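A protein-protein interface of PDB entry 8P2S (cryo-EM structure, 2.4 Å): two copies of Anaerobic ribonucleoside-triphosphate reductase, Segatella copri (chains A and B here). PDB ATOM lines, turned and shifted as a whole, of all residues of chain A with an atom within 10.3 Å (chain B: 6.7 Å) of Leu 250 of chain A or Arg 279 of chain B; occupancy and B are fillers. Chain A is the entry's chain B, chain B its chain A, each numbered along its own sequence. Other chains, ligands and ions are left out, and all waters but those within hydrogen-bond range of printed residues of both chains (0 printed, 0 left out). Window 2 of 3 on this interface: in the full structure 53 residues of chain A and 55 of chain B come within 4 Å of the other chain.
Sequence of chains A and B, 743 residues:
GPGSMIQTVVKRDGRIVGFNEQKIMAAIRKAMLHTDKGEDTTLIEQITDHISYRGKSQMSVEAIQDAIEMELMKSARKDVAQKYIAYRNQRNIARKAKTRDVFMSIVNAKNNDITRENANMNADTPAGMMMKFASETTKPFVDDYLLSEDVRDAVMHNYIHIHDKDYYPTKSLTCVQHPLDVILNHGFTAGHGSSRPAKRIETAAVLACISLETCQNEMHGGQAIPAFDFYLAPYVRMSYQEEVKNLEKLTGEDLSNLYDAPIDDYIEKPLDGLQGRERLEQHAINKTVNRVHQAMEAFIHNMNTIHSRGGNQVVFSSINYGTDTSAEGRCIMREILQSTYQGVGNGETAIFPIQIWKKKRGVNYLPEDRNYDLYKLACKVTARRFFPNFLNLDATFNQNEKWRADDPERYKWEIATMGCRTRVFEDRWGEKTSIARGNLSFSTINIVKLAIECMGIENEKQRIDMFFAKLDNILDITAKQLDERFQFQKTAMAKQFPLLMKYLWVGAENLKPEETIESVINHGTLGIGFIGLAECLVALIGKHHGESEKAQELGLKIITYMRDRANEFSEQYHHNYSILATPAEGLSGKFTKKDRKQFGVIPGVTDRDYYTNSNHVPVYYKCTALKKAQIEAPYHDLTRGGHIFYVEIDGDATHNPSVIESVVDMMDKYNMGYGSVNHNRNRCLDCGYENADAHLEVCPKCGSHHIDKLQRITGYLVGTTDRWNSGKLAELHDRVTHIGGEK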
ATOM      1  N   GLU A 242      -9.663 -13.416   8.542  1.00  0.00           N
ATOM      2  CA  GLU A 242      -9.244 -12.093   8.994  1.00  0.00           C
ATOM      3  C   GLU A 242      -7.739 -12.019   9.218  1.00  0.00           C
ATOM      4  O   GLU A 242      -7.102 -11.042   8.810  1.00  0.00           O
ATOM      5  CB  GLU A 242      -9.988 -11.713  10.274  1.00  0.00           C
ATOM      6  CG  GLU A 242     -11.475 -11.472  10.079  1.00  0.00           C
ATOM      7  CD  GLU A 242     -12.183 -11.126  11.373  1.00  0.00           C
ATOM      8  OE1 GLU A 242     -11.613 -11.389  12.452  1.00  0.00           O
ATOM      9  OE2 GLU A 242     -13.308 -10.588  11.311  1.00  0.00           O
ATOM     10  N   GLU A 243      -7.153 -13.042   9.843  1.00  0.00           N
ATOM     11  CA  GLU A 243      -5.703 -13.079   9.997  1.00  0.00           C
ATOM     12  C   GLU A 243      -4.980 -13.141   8.655  1.00  0.00           C
ATOM     13  O   GLU A 243      -3.960 -12.463   8.478  1.00  0.00           O
ATOM     14  CB  GLU A 243      -5.302 -14.267  10.870  1.00  0.00           C
ATOM     15  CG  GLU A 243      -4.769 -13.868  12.226  1.00  0.00           C
ATOM     16  CD  GLU A 243      -3.409 -13.197  12.140  1.00  0.00           C
ATOM     17  OE1 GLU A 243      -2.704 -13.406  11.129  1.00  0.00           O
ATOM     18  OE2 GLU A 243      -3.047 -12.461  13.081  1.00  0.00           O
ATOM     19  N   VAL A 244      -5.495 -13.919   7.710  1.00  0.00           N
ATOM     20  CA  VAL A 244      -4.904 -14.003   6.378  1.00  0.00           C
ATOM     21  C   VAL A 244      -4.961 -12.663   5.661  1.00  0.00           C
ATOM     22  O   VAL A 244      -3.990 -12.246   5.025  1.00  0.00           O
ATOM     23  CB  VAL A 244      -5.599 -15.113   5.561  1.00  0.00           C
ATOM     24  CG1 VAL A 244      -5.212 -15.017   4.101  1.00  0.00           C
ATOM     25  CG2 VAL A 244      -5.230 -16.479   6.112  1.00  0.00           C
ATOM     26  N   LYS A 245      -6.091 -11.958   5.747  1.00  0.00           N
ATOM     27  CA  LYS A 245      -6.190 -10.666   5.074  1.00  0.00           C
ATOM     28  C   LYS A 245      -5.324  -9.616   5.764  1.00  0.00           C
ATOM     29  O   LYS A 245      -4.802  -8.708   5.108  1.00  0.00           O
ATOM     30  CB  LYS A 245      -7.647 -10.211   4.987  1.00  0.00           C
ATOM     31  CG  LYS A 245      -8.262  -9.736   6.282  1.00  0.00           C
ATOM     32  CD  LYS A 245      -9.624  -9.105   6.041  1.00  0.00           C
ATOM     33  CE  LYS A 245     -10.553 -10.062   5.311  1.00  0.00           C
ATOM     34  NZ  LYS A 245     -10.806 -11.298   6.100  1.00  0.00           N
ATOM     35  N   ASN A 246      -5.137  -9.730   7.082  1.00  0.00           N
ATOM     36  CA  ASN A 246      -4.195  -8.851   7.767  1.00  0.00           C
ATOM     37  C   ASN A 246      -2.773  -9.083   7.269  1.00  0.00           C
ATOM     38  O   ASN A 246      -2.029  -8.133   6.997  1.00  0.00           O
ATOM     39  CB  ASN A 246      -4.277  -9.060   9.281  1.00  0.00           C
ATOM     40  CG  ASN A 246      -5.511  -8.428   9.891  1.00  0.00           C
ATOM     41  OD1 ASN A 246      -6.244  -9.070  10.644  1.00  0.00           O
ATOM     42  ND2 ASN A 246      -5.747  -7.161   9.570  1.00  0.00           N
ATOM     43  N   LEU A 247      -2.374 -10.353   7.150  1.00  0.00           N
ATOM     44  CA  LEU A 247      -1.052 -10.654   6.603  1.00  0.00           C
ATOM     45  C   LEU A 247      -0.923 -10.173   5.164  1.00  0.00           C
ATOM     46  O   LEU A 247       0.150  -9.719   4.753  1.00  0.00           O
ATOM     47  CB  LEU A 247      -0.768 -12.153   6.683  1.00  0.00           C
ATOM     48  CG  LEU A 247      -0.603 -12.769   8.071  1.00  0.00           C
ATOM     49  CD1 LEU A 247      -0.229 -14.234   7.953  1.00  0.00           C
ATOM     50  CD2 LEU A 247       0.433 -12.012   8.881  1.00  0.00           C
ATOM     51  N   GLU A 248      -2.002 -10.270   4.388  1.00  0.00           N
ATOM     52  CA  GLU A 248      -1.981  -9.800   3.008  1.00  0.00           C
ATOM     53  C   GLU A 248      -1.814  -8.287   2.939  1.00  0.00           C
ATOM     54  O   GLU A 248      -1.098  -7.776   2.072  1.00  0.00           O
ATOM     55  CB  GLU A 248      -3.261 -10.240   2.299  1.00  0.00           C
ATOM     56  CG  GLU A 248      -3.338  -9.864   0.836  1.00  0.00           C
ATOM     57  CD  GLU A 248      -4.524 -10.504   0.146  1.00  0.00           C
ATOM     58  OE1 GLU A 248      -5.272 -11.243   0.821  1.00  0.00           O
ATOM     59  OE2 GLU A 248      -4.710 -10.273  -1.068  1.00  0.00           O
ATOM     60  N   LYS A 249      -2.478  -7.555   3.835  1.00  0.00           N
ATOM     61  CA  LYS A 249      -2.283  -6.110   3.895  1.00  0.00           C
ATOM     62  C   LYS A 249      -0.859  -5.764   4.310  1.00  0.00           C
ATOM     63  O   LYS A 249      -0.263  -4.817   3.784  1.00  0.00           O
ATOM     64  CB  LYS A 249      -3.289  -5.478   4.857  1.00  0.00           C
ATOM     65  CG  LYS A 249      -4.719  -5.489   4.350  1.00  0.00           C
ATOM     66  CD  LYS A 249      -5.654  -4.795   5.324  1.00  0.00           C
ATOM     67  CE  LYS A 249      -7.090  -4.820   4.824  1.00  0.00           C
ATOM     68  NZ  LYS A 249      -7.234  -4.139   3.508  1.00  0.00           N
ATOM     69  N   LEU A 250      -0.300  -6.516   5.261  1.00  0.00           N
ATOM     70  CA  LEU A 250       1.066  -6.249   5.699  1.00  0.00           C
ATOM     71  C   LEU A 250       2.076  -6.508   4.586  1.00  0.00           C
ATOM     72  O   LEU A 250       3.009  -5.722   4.391  1.00  0.00           O
ATOM     73  CB  LEU A 250       1.402  -7.096   6.925  1.00  0.00           C
ATOM     74  CG  LEU A 250       2.828  -6.931   7.449  1.00  0.00           C
ATOM     75  CD1 LEU A 250       3.081  -5.488   7.856  1.00  0.00           C
ATOM     76  CD2 LEU A 250       3.093  -7.873   8.609  1.00  0.00           C
ATOM     77  N   THR A 251       1.905  -7.602   3.843  1.00  0.00           N
ATOM     78  CA  THR A 251       2.915  -8.045   2.890  1.00  0.00           C
ATOM     79  C   THR A 251       2.585  -7.706   1.442  1.00  0.00           C
ATOM     80  O   THR A 251       3.507  -7.556   0.634  1.00  0.00           O
ATOM     81  CB  THR A 251       3.124  -9.560   3.010  1.00  0.00           C
ATOM     82  OG1 THR A 251       3.145  -9.930   4.393  1.00  0.00           O
ATOM     83  CG2 THR A 251       4.444  -9.973   2.375  1.00  0.00           C
ATOM     84  N   GLY A 252       1.309  -7.567   1.096  1.00  0.00           N
ATOM     85  CA  GLY A 252       0.941  -7.293  -0.276  1.00  0.00           C
ATOM     86  C   GLY A 252       0.868  -8.506  -1.174  1.00  0.00           C
ATOM     87  O   GLY A 252       0.703  -8.347  -2.388  1.00  0.00           O
ATOM     88  N   GLU A 253       0.985  -9.710  -0.619  1.00  0.00           N
ATOM     89  CA  GLU A 253       0.911 -10.924  -1.416  1.00  0.00           C
ATOM     90  C   GLU A 253      -0.525 -11.167  -1.880  1.00  0.00           C
ATOM     91  O   GLU A 253      -1.436 -10.373  -1.635  1.00  0.00           O
ATOM     92  CB  GLU A 253       1.428 -12.117  -0.617  1.00  0.00           C
ATOM     93  CG  GLU A 253       2.887 -12.023  -0.219  1.00  0.00           C
ATOM     94  CD  GLU A 253       3.383 -13.284   0.466  1.00  0.00           C
ATOM     95  OE1 GLU A 253       2.603 -14.254   0.565  1.00  0.00           O
ATOM     96  OE2 GLU A 253       4.552 -13.304   0.903  1.00  0.00           O
ATOM     97  N   ASP A 254      -0.723 -12.285  -2.570  1.00  0.00           N
ATOM     98  CA  ASP A 254      -2.039 -12.714  -3.039  1.00  0.00           C
ATOM     99  C   ASP A 254      -2.373 -14.012  -2.311  1.00  0.00           C
ATOM    100  O   ASP A 254      -2.100 -15.108  -2.804  1.00  0.00           O
ATOM    101  CB  ASP A 254      -2.054 -12.895  -4.554  1.00  0.00           C
ATOM    102  CG  ASP A 254      -3.446 -13.162  -5.097  1.00  0.00           C
ATOM    103  OD1 ASP A 254      -4.421 -13.062  -4.321  1.00  0.00           O
ATOM    104  OD2 ASP A 254      -3.567 -13.472  -6.300  1.00  0.00           O
ATOM    105  N   LEU A 255      -2.975 -13.880  -1.128  1.00  0.00           N
ATOM    106  CA  LEU A 255      -3.353 -15.019  -0.303  1.00  0.00           C
ATOM    107  C   LEU A 255      -4.806 -15.423  -0.511  1.00  0.00           C
ATOM    108  O   LEU A 255      -5.451 -15.928   0.413  1.00  0.00           O
ATOM    109  CB  LEU A 255      -3.094 -14.711   1.171  1.00  0.00           C
ATOM    110  CG  LEU A 255      -1.690 -14.224   1.531  1.00  0.00           C
ATOM    111  CD1 LEU A 255      -1.548 -14.033   3.031  1.00  0.00           C
ATOM    112  CD2 LEU A 255      -0.647 -15.188   1.014  1.00  0.00           C
ATOM    113  N   TYR A 259      -8.129 -18.664   1.581  1.00  0.00           N
ATOM    114  CA  TYR A 259      -9.392 -18.225   2.159  1.00  0.00           C
ATOM    115  C   TYR A 259     -10.333 -19.383   2.449  1.00  0.00           C
ATOM    116  O   TYR A 259     -10.826 -19.515   3.574  1.00  0.00           O
ATOM    117  CB  TYR A 259     -10.084 -17.220   1.227  1.00  0.00           C
ATOM    118  CG  TYR A 259      -9.479 -15.836   1.248  1.00  0.00           C
ATOM    119  CD1 TYR A 259      -8.687 -15.420   2.307  1.00  0.00           C
ATOM    120  CD2 TYR A 259      -9.704 -14.944   0.209  1.00  0.00           C
ATOM    121  CE1 TYR A 259      -8.135 -14.158   2.331  1.00  0.00           C
ATOM    122  CE2 TYR A 259      -9.155 -13.678   0.224  1.00  0.00           C
ATOM    123  CZ  TYR A 259      -8.372 -13.291   1.286  1.00  0.00           C
ATOM    124  OH  TYR A 259      -7.823 -12.031   1.305  1.00  0.00           O
ATOM    125  N   LEU A 280       3.767 -17.860   6.445  1.00  0.00           N
ATOM    126  CA  LEU A 280       2.632 -16.962   6.606  1.00  0.00           C
ATOM    127  C   LEU A 280       1.378 -17.745   6.949  1.00  0.00           C
ATOM    128  O   LEU A 280       0.712 -17.456   7.953  1.00  0.00           O
ATOM    129  CB  LEU A 280       2.420 -16.141   5.334  1.00  0.00           C
ATOM    130  CG  LEU A 280       3.163 -14.812   5.185  1.00  0.00           C
ATOM    131  CD1 LEU A 280       4.672 -14.996   5.232  1.00  0.00           C
ATOM    132  CD2 LEU A 280       2.750 -14.136   3.891  1.00  0.00           C
ATOM    133  N   HIS A 283       1.461 -18.984  10.399  1.00  0.00           N
ATOM    134  CA  HIS A 283       1.283 -17.880  11.330  1.00  0.00           C
ATOM    135  C   HIS A 283      -0.194 -17.607  11.555  1.00  0.00           C
ATOM    136  O   HIS A 283      -0.642 -17.483  12.702  1.00  0.00           O
ATOM    137  CB  HIS A 283       1.995 -16.633  10.811  1.00  0.00           C
ATOM    138  CG  HIS A 283       2.061 -15.518  11.807  1.00  0.00           C
ATOM    139  ND1 HIS A 283       2.862 -15.567  12.926  1.00  0.00           N
ATOM    140  CD2 HIS A 283       1.419 -14.327  11.857  1.00  0.00           C
ATOM    141  CE1 HIS A 283       2.715 -14.453  13.619  1.00  0.00           C
ATOM    142  NE2 HIS A 283       1.844 -13.684  12.992  1.00  0.00           N
ATOM    143  N   LEU B 247       4.360  -9.437  15.162  1.00  0.00           N
ATOM    144  CA  LEU B 247       5.121  -9.068  13.976  1.00  0.00           C
ATOM    145  C   LEU B 247       6.575  -9.516  14.053  1.00  0.00           C
ATOM    146  O   LEU B 247       7.138  -9.912  13.028  1.00  0.00           O
ATOM    147  CB  LEU B 247       5.055  -7.558  13.753  1.00  0.00           C
ATOM    148  CG  LEU B 247       3.668  -6.981  13.472  1.00  0.00           C
ATOM    149  CD1 LEU B 247       3.755  -5.484  13.278  1.00  0.00           C
ATOM    150  CD2 LEU B 247       3.049  -7.644  12.257  1.00  0.00           C
ATOM    151  N   LEU B 250       6.623 -13.191  13.371  1.00  0.00           N
ATOM    152  CA  LEU B 250       6.399 -13.368  11.941  1.00  0.00           C
ATOM    153  C   LEU B 250       7.647 -13.051  11.127  1.00  0.00           C
ATOM    154  O   LEU B 250       7.915 -13.718  10.121  1.00  0.00           O
ATOM    155  CB  LEU B 250       5.233 -12.489  11.485  1.00  0.00           C
ATOM    156  CG  LEU B 250       4.978 -12.373   9.983  1.00  0.00           C
ATOM    157  CD1 LEU B 250       4.553 -13.709   9.395  1.00  0.00           C
ATOM    158  CD2 LEU B 250       3.937 -11.306   9.705  1.00  0.00           C
ATOM    159  N   THR B 251       8.425 -12.050  11.545  1.00  0.00           N
ATOM    160  CA  THR B 251       9.538 -11.558  10.743  1.00  0.00           C
ATOM    161  C   THR B 251      10.918 -11.817  11.333  1.00  0.00           C
ATOM    162  O   THR B 251      11.901 -11.733  10.589  1.00  0.00           O
ATOM    163  CB  THR B 251       9.394 -10.047  10.501  1.00  0.00           C
ATOM    164  OG1 THR B 251       9.465  -9.355  11.753  1.00  0.00           O
ATOM    165  CG2 THR B 251       8.065  -9.734   9.832  1.00  0.00           C
ATOM    166  N   PRO B 270      -3.238   4.842   5.756  1.00  0.00           N
ATOM    167  CA  PRO B 270      -3.502   3.860   4.689  1.00  0.00           C
ATOM    168  C   PRO B 270      -2.406   2.825   4.489  1.00  0.00           C
ATOM    169  O   PRO B 270      -2.682   1.776   3.892  1.00  0.00           O
ATOM    170  CB  PRO B 270      -3.680   4.740   3.443  1.00  0.00           C
ATOM    171  CG  PRO B 270      -3.012   6.030   3.779  1.00  0.00           C
ATOM    172  CD  PRO B 270      -3.257   6.221   5.239  1.00  0.00           C
ATOM    173  N   LEU B 271      -1.177   3.085   4.939  1.00  0.00           N
ATOM    174  CA  LEU B 271      -0.045   2.172   4.775  1.00  0.00           C
ATOM    175  C   LEU B 271       0.313   1.944   3.308  1.00  0.00           C
ATOM    176  O   LEU B 271       0.801   0.871   2.944  1.00  0.00           O
ATOM    177  CB  LEU B 271      -0.314   0.827   5.470  1.00  0.00           C
ATOM    178  CG  LEU B 271       0.828  -0.120   5.849  1.00  0.00           C
ATOM    179  CD1 LEU B 271       1.709   0.492   6.920  1.00  0.00           C
ATOM    180  CD2 LEU B 271       0.274  -1.458   6.309  1.00  0.00           C
ATOM    181  N   ASP B 272       0.077   2.938   2.448  1.00  0.00           N
ATOM    182  CA  ASP B 272       0.254   2.742   1.012  1.00  0.00           C
ATOM    183  C   ASP B 272       1.721   2.536   0.647  1.00  0.00           C
ATOM    184  O   ASP B 272       2.072   1.570  -0.041  1.00  0.00           O
ATOM    185  CB  ASP B 272      -0.324   3.935   0.253  1.00  0.00           C
ATOM    186  CG  ASP B 272      -1.802   4.139   0.525  1.00  0.00           C
ATOM    187  OD1 ASP B 272      -2.521   3.132   0.686  1.00  0.00           O
ATOM    188  OD2 ASP B 272      -2.244   5.306   0.580  1.00  0.00           O
ATOM    189  N   GLY B 273       2.592   3.435   1.100  1.00  0.00           N
ATOM    190  CA  GLY B 273       3.978   3.445   0.673  1.00  0.00           C
ATOM    191  C   GLY B 273       4.990   3.537   1.794  1.00  0.00           C
ATOM    192  O   GLY B 273       6.018   4.205   1.651  1.00  0.00           O
ATOM    193  N   LEU B 274       4.722   2.870   2.913  1.00  0.00           N
ATOM    194  CA  LEU B 274       5.488   3.045   4.141  1.00  0.00           C
ATOM    195  C   LEU B 274       6.410   1.863   4.432  1.00  0.00           C
ATOM    196  O   LEU B 274       6.563   1.457   5.583  1.00  0.00           O
ATOM    197  CB  LEU B 274       4.549   3.280   5.320  1.00  0.00           C
ATOM    198  CG  LEU B 274       3.468   4.341   5.113  1.00  0.00           C
ATOM    199  CD1 LEU B 274       2.571   4.434   6.334  1.00  0.00           C
ATOM    200  CD2 LEU B 274       4.086   5.696   4.793  1.00  0.00           C
ATOM    201  N   GLN B 275       7.060   1.318   3.402  1.00  0.00           N
ATOM    202  CA  GLN B 275       7.892   0.123   3.541  1.00  0.00           C
ATOM    203  C   GLN B 275       8.973   0.257   4.612  1.00  0.00           C
ATOM    204  O   GLN B 275       9.326   1.369   5.018  1.00  0.00           O
ATOM    205  CB  GLN B 275       8.546  -0.222   2.203  1.00  0.00           C
ATOM    206  CG  GLN B 275       9.599   0.780   1.756  1.00  0.00           C
ATOM    207  CD  GLN B 275      10.305   0.361   0.482  1.00  0.00           C
ATOM    208  OE1 GLN B 275      10.008  -0.686  -0.092  1.00  0.00           O
ATOM    209  NE2 GLN B 275      11.249   1.181   0.033  1.00  0.00           N
ATOM    210  N   GLY B 276       9.505  -0.872   5.065  1.00  0.00           N
ATOM    211  CA  GLY B 276      10.516  -0.900   6.103  1.00  0.00           C
ATOM    212  C   GLY B 276       9.934  -1.169   7.477  1.00  0.00           C
ATOM    213  O   GLY B 276       8.820  -1.673   7.632  1.00  0.00           O
ATOM    214  N   ARG B 277      10.724  -0.825   8.500  1.00  0.00           N
ATOM    215  CA  ARG B 277      10.224  -0.868   9.871  1.00  0.00           C
ATOM    216  C   ARG B 277       9.071   0.101  10.084  1.00  0.00           C
ATOM    217  O   ARG B 277       8.271  -0.093  11.007  1.00  0.00           O
ATOM    218  CB  ARG B 277      11.347  -0.555  10.859  1.00  0.00           C
ATOM    219  CG  ARG B 277      12.012  -1.778  11.465  1.00  0.00           C
ATOM    220  CD  ARG B 277      13.320  -1.406  12.136  1.00  0.00           C
ATOM    221  NE  ARG B 277      13.932  -2.533  12.827  1.00  0.00           N
ATOM    222  CZ  ARG B 277      13.984  -2.663  14.145  1.00  0.00           C
ATOM    223  NH1 ARG B 277      13.473  -1.746  14.950  1.00  0.00           N
ATOM    224  NH2 ARG B 277      14.566  -3.738  14.669  1.00  0.00           N
ATOM    225  N   GLU B 278       8.974   1.142   9.254  1.00  0.00           N
ATOM    226  CA  GLU B 278       7.824   2.034   9.310  1.00  0.00           C
ATOM    227  C   GLU B 278       6.536   1.278   9.020  1.00  0.00           C
ATOM    228  O   GLU B 278       5.509   1.512   9.670  1.00  0.00           O
ATOM    229  CB  GLU B 278       8.005   3.183   8.318  1.00  0.00           C
ATOM    230  CG  GLU B 278       9.267   4.003   8.533  1.00  0.00           C
ATOM    231  CD  GLU B 278       9.231   4.815   9.813  1.00  0.00           C
ATOM    232  OE1 GLU B 278       8.123   5.069  10.332  1.00  0.00           O
ATOM    233  OE2 GLU B 278      10.314   5.202  10.303  1.00  0.00           O
ATOM    234  N   ARG B 279       6.573   0.362   8.050  1.00  0.00           N
ATOM    235  CA  ARG B 279       5.394  -0.440   7.739  1.00  0.00           C
ATOM    236  C   ARG B 279       4.983  -1.290   8.931  1.00  0.00           C
ATOM    237  O   ARG B 279       3.798  -1.368   9.269  1.00  0.00           O
ATOM    238  CB  ARG B 279       5.664  -1.320   6.520  1.00  0.00           C
ATOM    239  CG  ARG B 279       4.417  -1.930   5.919  1.00  0.00           C
ATOM    240  CD  ARG B 279       4.725  -2.671   4.634  1.00  0.00           C
ATOM    241  NE  ARG B 279       3.510  -3.122   3.971  1.00  0.00           N
ATOM    242  CZ  ARG B 279       2.830  -2.405   3.087  1.00  0.00           C
ATOM    243  NH1 ARG B 279       3.232  -1.200   2.721  1.00  0.00           N
ATOM    244  NH2 ARG B 279       1.718  -2.909   2.560  1.00  0.00           N
ATOM    245  N   LEU B 280       5.952  -1.929   9.587  1.00  0.00           N
ATOM    246  CA  LEU B 280       5.632  -2.761  10.740  1.00  0.00           C
ATOM    247  C   LEU B 280       5.073  -1.929  11.886  1.00  0.00           C
ATOM    248  O   LEU B 280       4.094  -2.325  12.531  1.00  0.00           O
ATOM    249  CB  LEU B 280       6.870  -3.536  11.189  1.00  0.00           C
ATOM    250  CG  LEU B 280       7.443  -4.534  10.181  1.00  0.00           C
ATOM    251  CD1 LEU B 280       8.639  -5.252  10.775  1.00  0.00           C
ATOM    252  CD2 LEU B 280       6.382  -5.529   9.745  1.00  0.00           C
ATOM    253  N   GLU B 281       5.673  -0.766  12.151  1.00  0.00           N
ATOM    254  CA  GLU B 281       5.190   0.089  13.231  1.00  0.00           C
ATOM    255  C   GLU B 281       3.771   0.571  12.957  1.00  0.00           C
ATOM    256  O   GLU B 281       2.903   0.524  13.838  1.00  0.00           O
ATOM    257  CB  GLU B 281       6.136   1.275  13.422  1.00  0.00           C
ATOM    258  CG  GLU B 281       5.727   2.219  14.541  1.00  0.00           C
ATOM    259  CD  GLU B 281       6.688   3.380  14.702  1.00  0.00           C
ATOM    260  OE1 GLU B 281       7.676   3.447  13.939  1.00  0.00           O
ATOM    261  OE2 GLU B 281       6.456   4.226  15.591  1.00  0.00           O
ATOM    262  N   GLN B 282       3.510   1.025  11.729  1.00  0.00           N
ATOM    263  CA  GLN B 282       2.177   1.512  11.395  1.00  0.00           C
ATOM    264  C   GLN B 282       1.156   0.383  11.400  1.00  0.00           C
ATOM    265  O   GLN B 282       0.007   0.584  11.802  1.00  0.00           O
ATOM    266  CB  GLN B 282       2.198   2.218  10.040  1.00  0.00           C
ATOM    267  CG  GLN B 282       0.877   2.869   9.661  1.00  0.00           C
ATOM    268  CD  GLN B 282       0.434   3.918  10.660  1.00  0.00           C
ATOM    269  OE1 GLN B 282       1.257   4.550  11.320  1.00  0.00           O
ATOM    270  NE2 GLN B 282      -0.873   4.104  10.780  1.00  0.00           N
ATOM    271  N   HIS B 283       1.550  -0.812  10.957  1.00  0.00           N
ATOM    272  CA  HIS B 283       0.642  -1.953  10.999  1.00  0.00           C
ATOM    273  C   HIS B 283       0.306  -2.333  12.435  1.00  0.00           C
ATOM    274  O   HIS B 283      -0.847  -2.658  12.747  1.00  0.00           O
ATOM    275  CB  HIS B 283       1.260  -3.134  10.251  1.00  0.00           C
ATOM    276  CG  HIS B 283       0.335  -4.299  10.090  1.00  0.00           C
ATOM    277  ND1 HIS B 283       0.431  -5.438  10.859  1.00  0.00           N
ATOM    278  CD2 HIS B 283      -0.702  -4.502   9.244  1.00  0.00           C
ATOM    279  CE1 HIS B 283      -0.508  -6.291  10.495  1.00  0.00           C
ATOM    280  NE2 HIS B 283      -1.210  -5.749   9.518  1.00  0.00           N
ATOM    281  N   ALA B 284       1.300  -2.298  13.326  1.00  0.00           N
ATOM    282  CA  ALA B 284       1.036  -2.566  14.735  1.00  0.00           C
ATOM    283  C   ALA B 284       0.103  -1.518  15.329  1.00  0.00           C
ATOM    284  O   ALA B 284      -0.802  -1.849  16.104  1.00  0.00           O
ATOM    285  CB  ALA B 284       2.350  -2.619  15.509  1.00  0.00           C
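Leu 247 of chain A touches Leu 250 of chain B, and with the chains exchanged Leu 250 of chain A touches Leu 247 of chain B.
Leu 250 of chain B touches its own counterpart, Leu 250 of chain A.
Leu 250 of chain A touches Leu 280 of chain B, but with the chains exchanged Leu 280 of chain A does not touch Leu 250 of chain B (4.4 Å).
Leu 250 of chain A touches His 283 of chain B, and with the chains exchanged His 283 of chain A touches Leu 250 of chain B.
Positions printed for both chains: 247, 250, 251, 280 and 283.
Of the 9 pairs that touch across the chains among the printed residues, 5 have their exchanged pair printed and touching as well.
Hydrophobic or aromatic side chains of chain A within 4 Å of the printed part of chain B: Leu 247, Leu 250 and His 283.
Printed residues of chain B that touch a printed residue of chain A: Leu 247, Leu 250, Arg 279, Leu 280 and His 283.
Hydrophobic or aromatic side chains of chain B that line the printed part of chain A: Leu 247, Leu 250, Leu 280 and His 283.
Among the printed residues, no Asp or Glu carboxylate lies within 4 Å of a Lys or Arg side-chain nitrogen of the other chain.
Among the printed residues, merely in contact across the chains: Asn 246 of chain A with His 283 of chain B, Leu 250 of chain A with Leu 247 of chain B, Leu 247 of chain A with Leu 250 of chain B, Leu 250 of chain A with Leu 250 of chain B, Leu 250 of chain A with His 283 of chain B, Leu 250 of chain A with Leu 280 of chain B and His 283 of chain A with Leu 250 of chain B.
The backbone carbonyl oxygen (O) of Leu 247 of chain B sits at hydrogen-bond distance from the side-chain hydroxyl (OG1) of Thr 251 of chain B, 2.7 Å away.
The guanidinium group (NH1) of Arg 279 of chain B is in hydrogen-bond range of the backbone carbonyl oxygen (O) of Leu 271 of chain B, 3.2 Å away.
O of Leu 274 of chain B sits at hydrogen-bond distance from N of Arg 279 of chain B.
The backbone carbonyl oxygen (O) of Glu 242 of chain A lies close to the side-chain amide oxygen (OD1) of Asn 246 of chain A (2.8 Å).
O of Leu 247 of chain A lies within hydrogen-bond range of OG1 of Thr 251 of chain A (3.0 Å).
The guanidinium group (NH2) of Arg 279 of chain B is in hydrogen-bond range of the backbone carbonyl oxygen (O) of Lys 249 of chain A.
O of Leu 250 of chain A sits at hydrogen-bond distance from NE of Arg 279 of chain B.
Leu 250 of chain A touches just these residues of chain B: Leu 247, Leu 250, Arg 279, Leu 280 and His 283.
Of chain A, only Lys 249 (3.0 Å) and Leu 250 (2.7 Å) come within 4 Å of Arg 279 of chain B.
Gly 276 of chain B touches none of the printed residues of chain A.
Of chain A, only Leu 250 (3.8 Å) comes within 4 Å of Leu 280 of chain B.
Of chain A, only Asn 246 and Leu 250 come within 4 Å of His 283 of chain B.
Of the printed residues of chain B, His 283 of chain A touches Leu 250 (3.8 Å).
Printed residues of chain B within 4 Å of Leu 247 of chain A: Leu 250.
Printed residues of chain B within 4 Å of Lys 249 of chain A: Arg 279 (3.0 Å).
Of the printed residues of chain B, Asn 246 of chain A touches His 283 (3.6 Å).
Glu 248 of chain A touches none of the printed residues of chain B.
The nearest residue of chain A that does not touch Arg 279 of chain B is Thr 251 of chain A (4.8 Å).
The nearest printed residue of chain B that does not touch Leu 247 of chain A is His 283 of chain B (5.3 Å).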
